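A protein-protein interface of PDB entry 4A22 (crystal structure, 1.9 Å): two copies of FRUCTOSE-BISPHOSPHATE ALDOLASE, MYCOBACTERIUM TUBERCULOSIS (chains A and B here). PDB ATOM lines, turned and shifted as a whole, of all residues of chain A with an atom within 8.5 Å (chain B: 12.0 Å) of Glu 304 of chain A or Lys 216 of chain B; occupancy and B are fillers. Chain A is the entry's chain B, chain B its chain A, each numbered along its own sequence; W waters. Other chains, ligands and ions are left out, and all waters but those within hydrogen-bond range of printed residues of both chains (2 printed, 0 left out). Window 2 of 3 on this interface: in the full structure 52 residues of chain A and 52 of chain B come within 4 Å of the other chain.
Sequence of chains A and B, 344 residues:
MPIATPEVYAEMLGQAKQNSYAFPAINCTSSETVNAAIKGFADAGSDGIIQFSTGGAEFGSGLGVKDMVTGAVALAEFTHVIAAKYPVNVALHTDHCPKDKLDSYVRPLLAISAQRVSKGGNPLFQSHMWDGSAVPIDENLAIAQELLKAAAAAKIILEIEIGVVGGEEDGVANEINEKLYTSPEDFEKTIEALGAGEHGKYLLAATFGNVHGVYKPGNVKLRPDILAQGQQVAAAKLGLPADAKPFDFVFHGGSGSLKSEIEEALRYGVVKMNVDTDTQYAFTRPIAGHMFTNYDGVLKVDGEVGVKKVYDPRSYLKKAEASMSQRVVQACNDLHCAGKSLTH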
ATOM      1  N   ASP A 296     -18.772  -0.221  -0.462  1.00  0.00           N
ATOM      2  CA  ASP A 296     -20.006   0.031   0.265  1.00  0.00           C
ATOM      3  C   ASP A 296     -20.188   1.526   0.555  1.00  0.00           C
ATOM      4  O   ASP A 296     -21.149   1.907   1.212  1.00  0.00           O
ATOM      5  CB  ASP A 296     -20.039  -0.793   1.558  1.00  0.00           C
ATOM      6  CG  ASP A 296     -18.912  -0.439   2.511  1.00  0.00           C
ATOM      7  OD1 ASP A 296     -17.893   0.143   2.064  1.00  0.00           O
ATOM      8  OD2 ASP A 296     -19.052  -0.732   3.717  1.00  0.00           O
ATOM      9  N   GLY A 297     -19.233   2.361   0.125  1.00  0.00           N
ATOM     10  CA  GLY A 297     -19.440   3.803   0.127  1.00  0.00           C
ATOM     11  C   GLY A 297     -19.797   4.383  -1.226  1.00  0.00           C
ATOM     12  O   GLY A 297     -20.606   5.304  -1.305  1.00  0.00           O
ATOM     13  N   LEU A 299     -21.341   2.591  -3.471  1.00  0.00           N
ATOM     14  CA  LEU A 299     -22.648   2.004  -3.766  1.00  0.00           C
ATOM     15  C   LEU A 299     -23.565   2.259  -2.579  1.00  0.00           C
ATOM     16  O   LEU A 299     -23.101   2.296  -1.444  1.00  0.00           O
ATOM     17  CB  LEU A 299     -22.547   0.493  -4.001  1.00  0.00           C
ATOM     18  CG  LEU A 299     -21.710   0.084  -5.207  1.00  0.00           C
ATOM     19  CD1 LEU A 299     -21.646  -1.440  -5.313  1.00  0.00           C
ATOM     20  CD2 LEU A 299     -22.278   0.731  -6.480  1.00  0.00           C
ATOM     21  N   LYS A 300     -24.856   2.420  -2.842  1.00  0.00           N
ATOM     22  CA  LYS A 300     -25.828   2.519  -1.759  1.00  0.00           C
ATOM     23  C   LYS A 300     -26.248   1.080  -1.496  1.00  0.00           C
ATOM     24  O   LYS A 300     -26.975   0.469  -2.280  1.00  0.00           O
ATOM     25  CB  LYS A 300     -27.000   3.399  -2.198  1.00  0.00           C
ATOM     26  CG  LYS A 300     -26.536   4.831  -2.529  1.00  0.00           C
ATOM     27  CD  LYS A 300     -27.652   5.732  -3.052  1.00  0.00           C
ATOM     28  CE  LYS A 300     -27.219   7.200  -3.017  1.00  0.00           C
ATOM     29  NZ  LYS A 300     -28.273   8.134  -3.500  1.00  0.00           N
ATOM     30  N   VAL A 301     -25.771   0.556  -0.378  1.00  0.00           N
ATOM     31  CA  VAL A 301     -25.867  -0.878  -0.089  1.00  0.00           C
ATOM     32  C   VAL A 301     -26.684  -1.151   1.167  1.00  0.00           C
ATOM     33  O   VAL A 301     -26.586  -0.414   2.158  1.00  0.00           O
ATOM     34  CB  VAL A 301     -24.481  -1.506   0.117  1.00  0.00           C
ATOM     35  CG1 VAL A 301     -24.619  -2.983   0.409  1.00  0.00           C
ATOM     36  CG2 VAL A 301     -23.595  -1.270  -1.124  1.00  0.00           C
ATOM     37  N   ASP A 302     -27.475  -2.224   1.113  1.00  0.00           N
ATOM     38  CA  ASP A 302     -28.228  -2.696   2.273  1.00  0.00           C
ATOM     39  C   ASP A 302     -29.037  -1.562   2.896  1.00  0.00           C
ATOM     40  O   ASP A 302     -29.117  -1.458   4.120  1.00  0.00           O
ATOM     41  CB  ASP A 302     -27.270  -3.302   3.314  1.00  0.00           C
ATOM     42  CG  ASP A 302     -26.645  -4.629   2.855  1.00  0.00           C
ATOM     43  OD1 ASP A 302     -27.348  -5.445   2.212  1.00  0.00           O
ATOM     44  OD2 ASP A 302     -25.450  -4.863   3.154  1.00  0.00           O
ATOM     45  N   GLY A 303     -29.634  -0.724   2.047  1.00  0.00           N
ATOM     46  CA  GLY A 303     -30.481   0.377   2.489  1.00  0.00           C
ATOM     47  C   GLY A 303     -29.746   1.609   3.035  1.00  0.00           C
ATOM     48  O   GLY A 303     -30.398   2.562   3.479  1.00  0.00           O
ATOM     49  N   GLU A 304     -28.410   1.586   3.060  1.00  0.00           N
ATOM     50  CA  GLU A 304     -27.614   2.781   3.389  1.00  0.00           C
ATOM     51  C   GLU A 304     -27.491   3.744   2.186  1.00  0.00           C
ATOM     52  O   GLU A 304     -27.711   3.347   1.045  1.00  0.00           O
ATOM     53  CB  GLU A 304     -26.229   2.387   3.929  1.00  0.00           C
ATOM     54  CG  GLU A 304     -26.271   1.604   5.260  1.00  0.00           C
ATOM     55  CD  GLU A 304     -26.668   2.478   6.448  1.00  0.00           C
ATOM     56  OE1 GLU A 304     -25.828   3.276   6.925  1.00  0.00           O
ATOM     57  OE2 GLU A 304     -27.831   2.373   6.895  1.00  0.00           O
ATOM     58  N   VAL A 305     -27.167   5.009   2.440  1.00  0.00           N
ATOM     59  CA  VAL A 305     -27.100   6.007   1.362  1.00  0.00           C
ATOM     60  C   VAL A 305     -25.719   6.220   0.736  1.00  0.00           C
ATOM     61  O   VAL A 305     -25.523   7.169  -0.026  1.00  0.00           O
ATOM     62  CB  VAL A 305     -27.692   7.366   1.788  1.00  0.00           C
ATOM     63  CG1 VAL A 305     -29.172   7.197   2.124  1.00  0.00           C
ATOM     64  CG2 VAL A 305     -26.923   7.952   2.959  1.00  0.00           C
ATOM     65  N   GLY A 306     -24.755   5.378   1.080  1.00  0.00           N
ATOM     66  CA  GLY A 306     -23.417   5.501   0.522  1.00  0.00           C
ATOM     67  C   GLY A 306     -22.632   6.533   1.304  1.00  0.00           C
ATOM     68  O   GLY A 306     -23.126   7.059   2.309  1.00  0.00           O
ATOM     69  N   VAL A 307     -21.419   6.832   0.853  1.00  0.00           N
ATOM     70  CA  VAL A 307     -20.577   7.793   1.548  1.00  0.00           C
ATOM     71  C   VAL A 307     -20.099   8.841   0.543  1.00  0.00           C
ATOM     72  O   VAL A 307     -19.264   8.564  -0.320  1.00  0.00           O
ATOM     73  CB  VAL A 307     -19.362   7.093   2.210  1.00  0.00           C
ATOM     74  CG1 VAL A 307     -18.446   8.102   2.859  1.00  0.00           C
ATOM     75  CG2 VAL A 307     -19.832   6.073   3.243  1.00  0.00           C
ATOM     76  N   TYR A 311     -17.767   8.826  -3.066  1.00  0.00           N
ATOM     77  CA  TYR A 311     -18.372   8.815  -4.396  1.00  0.00           C
ATOM     78  C   TYR A 311     -18.293  10.158  -5.097  1.00  0.00           C
ATOM     79  O   TYR A 311     -18.595  10.260  -6.301  1.00  0.00           O
ATOM     80  CB  TYR A 311     -19.787   8.198  -4.418  1.00  0.00           C
ATOM     81  CG  TYR A 311     -20.936   8.932  -3.764  1.00  0.00           C
ATOM     82  CD1 TYR A 311     -21.443  10.110  -4.297  1.00  0.00           C
ATOM     83  CD2 TYR A 311     -21.606   8.369  -2.674  1.00  0.00           C
ATOM     84  CE1 TYR A 311     -22.542  10.749  -3.718  1.00  0.00           C
ATOM     85  CE2 TYR A 311     -22.694   8.998  -2.091  1.00  0.00           C
ATOM     86  CZ  TYR A 311     -23.161  10.184  -2.610  1.00  0.00           C
ATOM     87  OH  TYR A 311     -24.260  10.789  -2.033  1.00  0.00           O
ATOM     88  N   GLY B 167     -24.776  20.608   6.882  1.00  0.00           N
ATOM     89  CA  GLY B 167     -24.017  19.529   6.278  1.00  0.00           C
ATOM     90  C   GLY B 167     -24.178  18.231   7.049  1.00  0.00           C
ATOM     91  O   GLY B 167     -23.235  17.446   7.184  1.00  0.00           O
ATOM     92  N   GLY B 209     -34.030  25.364   6.018  1.00  0.00           N
ATOM     93  CA  GLY B 209     -33.827  24.004   6.494  1.00  0.00           C
ATOM     94  C   GLY B 209     -33.012  23.149   5.541  1.00  0.00           C
ATOM     95  O   GLY B 209     -32.805  21.966   5.782  1.00  0.00           O
ATOM     96  N   VAL B 211     -29.874  21.470   3.414  1.00  0.00           N
ATOM     97  CA  VAL B 211     -28.660  20.805   3.891  1.00  0.00           C
ATOM     98  C   VAL B 211     -27.835  20.237   2.730  1.00  0.00           C
ATOM     99  O   VAL B 211     -28.368  19.533   1.887  1.00  0.00           O
ATOM    100  CB  VAL B 211     -29.047  19.655   4.868  1.00  0.00           C
ATOM    101  CG1 VAL B 211     -27.864  18.702   5.127  1.00  0.00           C
ATOM    102  CG2 VAL B 211     -29.598  20.242   6.184  1.00  0.00           C
ATOM    103  N   HIS B 212     -26.540  20.543   2.675  1.00  0.00           N
ATOM    104  CA  HIS B 212     -25.667  19.948   1.659  1.00  0.00           C
ATOM    105  C   HIS B 212     -25.477  18.445   1.891  1.00  0.00           C
ATOM    106  O   HIS B 212     -25.211  18.021   3.015  1.00  0.00           O
ATOM    107  CB  HIS B 212     -24.303  20.630   1.661  1.00  0.00           C
ATOM    108  CG  HIS B 212     -24.310  21.997   1.053  1.00  0.00           C
ATOM    109  ND1 HIS B 212     -23.579  23.046   1.569  1.00  0.00           N
ATOM    110  CD2 HIS B 212     -24.949  22.485  -0.038  1.00  0.00           C
ATOM    111  CE1 HIS B 212     -23.771  24.122   0.827  1.00  0.00           C
ATOM    112  NE2 HIS B 212     -24.599  23.808  -0.154  1.00  0.00           N
ATOM    113  N   GLY B 213     -25.599  17.645   0.830  1.00  0.00           N
ATOM    114  CA  GLY B 213     -25.422  16.205   0.944  1.00  0.00           C
ATOM    115  C   GLY B 213     -26.727  15.438   0.852  1.00  0.00           C
ATOM    116  O   GLY B 213     -27.787  16.026   0.725  1.00  0.00           O
ATOM    117  N   VAL B 214     -26.652  14.115   0.916  1.00  0.00           N
ATOM    118  CA  VAL B 214     -27.829  13.266   0.761  1.00  0.00           C
ATOM    119  C   VAL B 214     -27.917  12.310   1.944  1.00  0.00           C
ATOM    120  O   VAL B 214     -26.952  11.613   2.257  1.00  0.00           O
ATOM    121  CB  VAL B 214     -27.775  12.463  -0.556  1.00  0.00           C
ATOM    122  CG1 VAL B 214     -28.697  11.252  -0.493  1.00  0.00           C
ATOM    123  CG2 VAL B 214     -28.132  13.360  -1.745  1.00  0.00           C
ATOM    124  N   TYR B 215     -29.078  12.283   2.596  1.00  0.00           N
ATOM    125  CA  TYR B 215     -29.243  11.548   3.848  1.00  0.00           C
ATOM    126  C   TYR B 215     -30.508  10.695   3.809  1.00  0.00           C
ATOM    127  O   TYR B 215     -31.325  10.824   2.894  1.00  0.00           O
ATOM    128  CB  TYR B 215     -29.281  12.530   5.025  1.00  0.00           C
ATOM    129  CG  TYR B 215     -28.111  13.477   4.993  1.00  0.00           C
ATOM    130  CD1 TYR B 215     -26.903  13.132   5.586  1.00  0.00           C
ATOM    131  CD2 TYR B 215     -28.197  14.697   4.328  1.00  0.00           C
ATOM    132  CE1 TYR B 215     -25.814  13.983   5.541  1.00  0.00           C
ATOM    133  CE2 TYR B 215     -27.115  15.557   4.278  1.00  0.00           C
ATOM    134  CZ  TYR B 215     -25.924  15.196   4.886  1.00  0.00           C
ATOM    135  OH  TYR B 215     -24.843  16.048   4.833  1.00  0.00           O
ATOM    136  N   LYS B 216     -30.658   9.807   4.785  1.00  0.00           N
ATOM    137  CA  LYS B 216     -31.847   8.972   4.845  1.00  0.00           C
ATOM    138  C   LYS B 216     -33.068   9.884   4.881  1.00  0.00           C
ATOM    139  O   LYS B 216     -33.222  10.683   5.807  1.00  0.00           O
ATOM    140  CB  LYS B 216     -31.799   8.049   6.065  1.00  0.00           C
ATOM    141  CG  LYS B 216     -30.675   7.025   5.987  1.00  0.00           C
ATOM    142  CD  LYS B 216     -30.877   5.879   6.960  1.00  0.00           C
ATOM    143  CE  LYS B 216     -30.318   4.580   6.397  1.00  0.00           C
ATOM    144  NZ  LYS B 216     -30.866   3.387   7.102  1.00  0.00           N
ATOM    145  N   PRO B 217     -33.937   9.775   3.861  1.00  0.00           N
ATOM    146  CA  PRO B 217     -35.040  10.723   3.658  1.00  0.00           C
ATOM    147  C   PRO B 217     -35.877  10.943   4.912  1.00  0.00           C
ATOM    148  O   PRO B 217     -36.207   9.989   5.616  1.00  0.00           O
ATOM    149  CB  PRO B 217     -35.869  10.058   2.555  1.00  0.00           C
ATOM    150  CG  PRO B 217     -34.881   9.248   1.796  1.00  0.00           C
ATOM    151  CD  PRO B 217     -33.914   8.732   2.820  1.00  0.00           C
ATOM    152  N   GLY B 218     -36.215  12.203   5.174  1.00  0.00           N
ATOM    153  CA  GLY B 218     -36.897  12.577   6.398  1.00  0.00           C
ATOM    154  C   GLY B 218     -35.942  13.226   7.383  1.00  0.00           C
ATOM    155  O   GLY B 218     -36.371  13.931   8.299  1.00  0.00           O
ATOM    156  N   ASN B 219     -34.643  12.984   7.201  1.00  0.00           N
ATOM    157  CA  ASN B 219     -33.617  13.632   8.014  1.00  0.00           C
ATOM    158  C   ASN B 219     -33.691  15.148   7.880  1.00  0.00           C
ATOM    159  O   ASN B 219     -33.768  15.867   8.877  1.00  0.00           O
ATOM    160  CB  ASN B 219     -32.212  13.159   7.618  1.00  0.00           C
ATOM    161  CG  ASN B 219     -31.815  11.859   8.292  1.00  0.00           C
ATOM    162  OD1 ASN B 219     -32.622  10.937   8.408  1.00  0.00           O
ATOM    163  ND2 ASN B 219     -30.566  11.780   8.751  1.00  0.00           N
ATOM    164  N   VAL B 220     -33.659  15.620   6.635  1.00  0.00           N
ATOM    165  CA  VAL B 220     -33.703  17.050   6.329  1.00  0.00           C
ATOM    166  C   VAL B 220     -35.141  17.592   6.348  1.00  0.00           C
ATOM    167  O   VAL B 220     -36.002  17.117   5.601  1.00  0.00           O
ATOM    168  CB  VAL B 220     -33.073  17.331   4.937  1.00  0.00           C
ATOM    169  CG1 VAL B 220     -33.208  18.801   4.569  1.00  0.00           C
ATOM    170  CG2 VAL B 220     -31.610  16.899   4.906  1.00  0.00           C
ATOM    171  N   LYS B 221     -35.394  18.585   7.202  1.00  0.00           N
ATOM    172  CA  LYS B 221     -36.723  19.194   7.310  1.00  0.00           C
ATOM    173  C   LYS B 221     -36.773  20.569   6.618  1.00  0.00           C
ATOM    174  O   LYS B 221     -36.235  21.547   7.131  1.00  0.00           O
ATOM    175  CB  LYS B 221     -37.133  19.329   8.793  1.00  0.00           C
ATOM    176  CG  LYS B 221     -36.229  20.257   9.618  1.00  0.00           C
ATOM    177  CD  LYS B 221     -36.649  20.367  11.107  1.00  0.00           C
ATOM    178  CE  LYS B 221     -35.690  21.233  11.971  1.00  0.00           C
ATOM    179  NZ  LYS B 221     -36.094  21.310  13.411  1.00  0.00           N
ATOM    180  N   LEU B 222     -37.438  20.644   5.467  1.00  0.00           N
ATOM    181  CA  LEU B 222     -37.570  21.906   4.737  1.00  0.00           C
ATOM    182  C   LEU B 222     -38.835  22.657   5.152  1.00  0.00           C
ATOM    183  O   LEU B 222     -39.870  22.044   5.399  1.00  0.00           O
ATOM    184  CB  LEU B 222     -37.592  21.652   3.229  1.00  0.00           C
ATOM    185  CG  LEU B 222     -36.323  20.991   2.702  1.00  0.00           C
ATOM    186  CD1 LEU B 222     -36.353  20.865   1.180  1.00  0.00           C
ATOM    187  CD2 LEU B 222     -35.083  21.779   3.163  1.00  0.00           C
ATOM    188  N   SER B 255     -30.120  18.079  -3.941  1.00  0.00           N
ATOM    189  CA  SER B 255     -30.066  16.623  -4.005  1.00  0.00           C
ATOM    190  C   SER B 255     -30.887  15.986  -2.888  1.00  0.00           C
ATOM    191  O   SER B 255     -30.923  16.500  -1.783  1.00  0.00           O
ATOM    192  CB  SER B 255     -28.610  16.164  -3.909  1.00  0.00           C
ATOM    193  OG  SER B 255     -27.866  16.710  -4.983  1.00  0.00           O
ATOM    194  N   GLY B 256     -31.556  14.875  -3.184  1.00  0.00           N
ATOM    195  CA  GLY B 256     -32.323  14.161  -2.176  1.00  0.00           C
ATOM    196  C   GLY B 256     -33.602  14.856  -1.738  1.00  0.00           C
ATOM    197  O   GLY B 256     -34.277  14.373  -0.834  1.00  0.00           O
ATOM    198  N   SER B 257     -33.951  15.973  -2.368  1.00  0.00           N
ATOM    199  CA  SER B 257     -35.164  16.692  -1.974  1.00  0.00           C
ATOM    200  C   SER B 257     -36.428  16.010  -2.505  1.00  0.00           C
ATOM    201  O   SER B 257     -36.403  15.355  -3.545  1.00  0.00           O
ATOM    202  CB  SER B 257     -35.097  18.153  -2.439  1.00  0.00           C
ATOM    203  OG  SER B 257     -33.908  18.774  -1.964  1.00  0.00           O
ATOM    204  N   LEU B 258     -37.531  16.170  -1.779  1.00  0.00           N
ATOM    205  CA  LEU B 258     -38.819  15.634  -2.203  1.00  0.00           C
ATOM    206  C   LEU B 258     -39.403  16.469  -3.331  1.00  0.00           C
ATOM    207  O   LEU B 258     -39.209  17.679  -3.376  1.00  0.00           O
ATOM    208  CB  LEU B 258     -39.797  15.641  -1.039  1.00  0.00           C
ATOM    209  CG  LEU B 258     -39.483  14.705   0.124  1.00  0.00           C
ATOM    210  CD1 LEU B 258     -40.709  14.652   1.036  1.00  0.00           C
ATOM    211  CD2 LEU B 258     -39.084  13.305  -0.383  1.00  0.00           C
ATOM    212  N   GLU B 261     -41.627  19.179  -1.872  1.00  0.00           N
ATOM    213  CA  GLU B 261     -40.841  20.271  -1.308  1.00  0.00           C
ATOM    214  C   GLU B 261     -40.456  21.246  -2.423  1.00  0.00           C
ATOM    215  O   GLU B 261     -40.566  22.466  -2.291  1.00  0.00           O
ATOM    216  CB  GLU B 261     -39.576  19.712  -0.647  1.00  0.00           C
ATOM    217  CG  GLU B 261     -39.838  18.860   0.601  1.00  0.00           C
ATOM    218  CD  GLU B 261     -38.579  18.165   1.132  1.00  0.00           C
ATOM    219  OE1 GLU B 261     -37.701  17.778   0.320  1.00  0.00           O
ATOM    220  OE2 GLU B 261     -38.467  18.010   2.370  1.00  0.00           O
ATOM    221  N   THR B 277     -24.613  16.550  -5.022  1.00  0.00           N
ATOM    222  CA  THR B 277     -24.471  15.190  -4.510  1.00  0.00           C
ATOM    223  C   THR B 277     -25.130  14.124  -5.381  1.00  0.00           C
ATOM    224  O   THR B 277     -24.534  13.094  -5.624  1.00  0.00           O
ATOM    225  CB  THR B 277     -25.043  15.107  -3.095  1.00  0.00           C
ATOM    226  OG1 THR B 277     -24.330  16.030  -2.261  1.00  0.00           O
ATOM    227  CG2 THR B 277     -24.899  13.681  -2.541  1.00  0.00           C
ATOM    228  N   ASP B 278     -26.356  14.367  -5.847  1.00  0.00           N
ATOM    229  CA  ASP B 278     -27.056  13.383  -6.671  1.00  0.00           C
ATOM    230  C   ASP B 278     -26.402  13.209  -8.037  1.00  0.00           C
ATOM    231  O   ASP B 278     -26.464  12.124  -8.610  1.00  0.00           O
ATOM    232  CB  ASP B 278     -28.517  13.769  -6.872  1.00  0.00           C
ATOM    233  CG  ASP B 278     -29.411  13.315  -5.711  1.00  0.00           C
ATOM    234  OD1 ASP B 278     -28.929  12.548  -4.853  1.00  0.00           O
ATOM    235  OD2 ASP B 278     -30.594  13.724  -5.663  1.00  0.00           O
ATOM    236  N   TYR B 281     -23.245  11.160  -7.411  1.00  0.00           N
ATOM    237  CA  TYR B 281     -23.543   9.740  -7.300  1.00  0.00           C
ATOM    238  C   TYR B 281     -23.833   9.170  -8.691  1.00  0.00           C
ATOM    239  O   TYR B 281     -23.384   8.083  -9.005  1.00  0.00           O
ATOM    240  CB  TYR B 281     -24.719   9.461  -6.357  1.00  0.00           C
ATOM    241  CG  TYR B 281     -24.943   7.966  -6.159  1.00  0.00           C
ATOM    242  CD1 TYR B 281     -24.090   7.227  -5.365  1.00  0.00           C
ATOM    243  CD2 TYR B 281     -25.990   7.303  -6.784  1.00  0.00           C
ATOM    244  CE1 TYR B 281     -24.270   5.869  -5.193  1.00  0.00           C
ATOM    245  CE2 TYR B 281     -26.181   5.947  -6.615  1.00  0.00           C
ATOM    246  CZ  TYR B 281     -25.315   5.232  -5.818  1.00  0.00           C
ATOM    247  OH  TYR B 281     -25.488   3.876  -5.630  1.00  0.00           O
ATOM    248  N   ARG B 285     -21.583   6.083 -10.112  1.00  0.00           N
ATOM    249  CA  ARG B 285     -22.244   4.769  -9.995  1.00  0.00           C
ATOM    250  C   ARG B 285     -21.880   3.795 -11.121  1.00  0.00           C
ATOM    251  O   ARG B 285     -21.523   2.650 -10.847  1.00  0.00           O
ATOM    252  CB  ARG B 285     -23.765   4.942  -9.909  1.00  0.00           C
ATOM    253  CG  ARG B 285     -24.554   3.633  -9.939  1.00  0.00           C
ATOM    254  CD  ARG B 285     -24.299   2.783  -8.706  1.00  0.00           C
ATOM    255  NE  ARG B 285     -25.038   1.527  -8.777  1.00  0.00           N
ATOM    256  CZ  ARG B 285     -24.647   0.471  -9.483  1.00  0.00           C
ATOM    257  NH1 ARG B 285     -23.509   0.507 -10.180  1.00  0.00           N
ATOM    258  NH2 ARG B 285     -25.397  -0.620  -9.503  1.00  0.00           N
HETATM  259  O   HOH W   1     -26.742  10.649  -3.587  1.00  0.00           O
HETATM  260  O   HOH W   2     -25.344   9.919   0.340  1.00  0.00           O
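Water W2 lies within hydrogen-bond range of OH of Tyr 311 of chain A (2.8 Å), O of Val 305 of chain A (2.8 Å) and O of Val 214 of chain B (3.0 Å).
Water W1 lies within hydrogen-bond range of OH of Tyr 311 of chain A, NZ of Lys 300 of chain A and OD1 of Asp 278 of chain B.
No position is printed for both chains.
Printed residues of chain A that touch a printed residue of chain B: Leu 299, Lys 300, Gly 303, Glu 304, Val 305 and Tyr 311.
Among the printed residues, Asp or Glu carboxylates within 4 Å of a Lys or Arg side-chain nitrogen of the other chain: Glu 304 of chain A with Lys 216 of chain B.
Among the printed residues, merely in contact across the chains: Tyr 311 of chain A with Thr 277 of chain B, Gly 303 of chain A with Lys 216 of chain B, Leu 299 of chain A with Arg 285 of chain B, Tyr 311 of chain A with Tyr 281 of chain B, Val 305 of chain A with Val 214 of chain B and Leu 299 of chain A with Tyr 281 of chain B.
The side-chain amino group (NZ) of Lys 216 of chain B lies within salt-bridge range of the side-chain carboxylate (OE2) of Glu 304 of chain A (3.2 Å).
N of Lys 300 of chain A sits at hydrogen-bond distance from OH of Tyr 281 of chain B (3.2 Å).
OG of Ser 255 of chain B is in hydrogen-bond range of N of Thr 277 of chain B.
The backbone carbonyl oxygen of Lys 216 of chain B lies close to the side-chain amide oxygen of Asn 219 of chain B, 2.7 Å away.
Glu 304 of chain A touches just one residue of chain B: Lys 216.
Printed residues of chain A within 4 Å of Lys 216 of chain B: Gly 303 and Glu 304.
Lys 300 of chain A touches just one residue of chain B: Tyr 281.
Asp 302 of chain A touches none of the printed residues of chain B.
Gly 306 of chain A touches none of the printed residues of chain B.
Printed residues of chain B within 4 Å of Leu 299 of chain A: Tyr 281 and Arg 285.
Printed residues of chain A within 4 Å of Val 214 of chain B: Val 305 (3.7 Å).
Of the printed residues of chain B, Val 305 of chain A touches Val 214 (3.7 Å).
The nearest printed residue of chain B that does not touch Leu 299 of chain A is Val 214 of chain B (10.6 Å).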
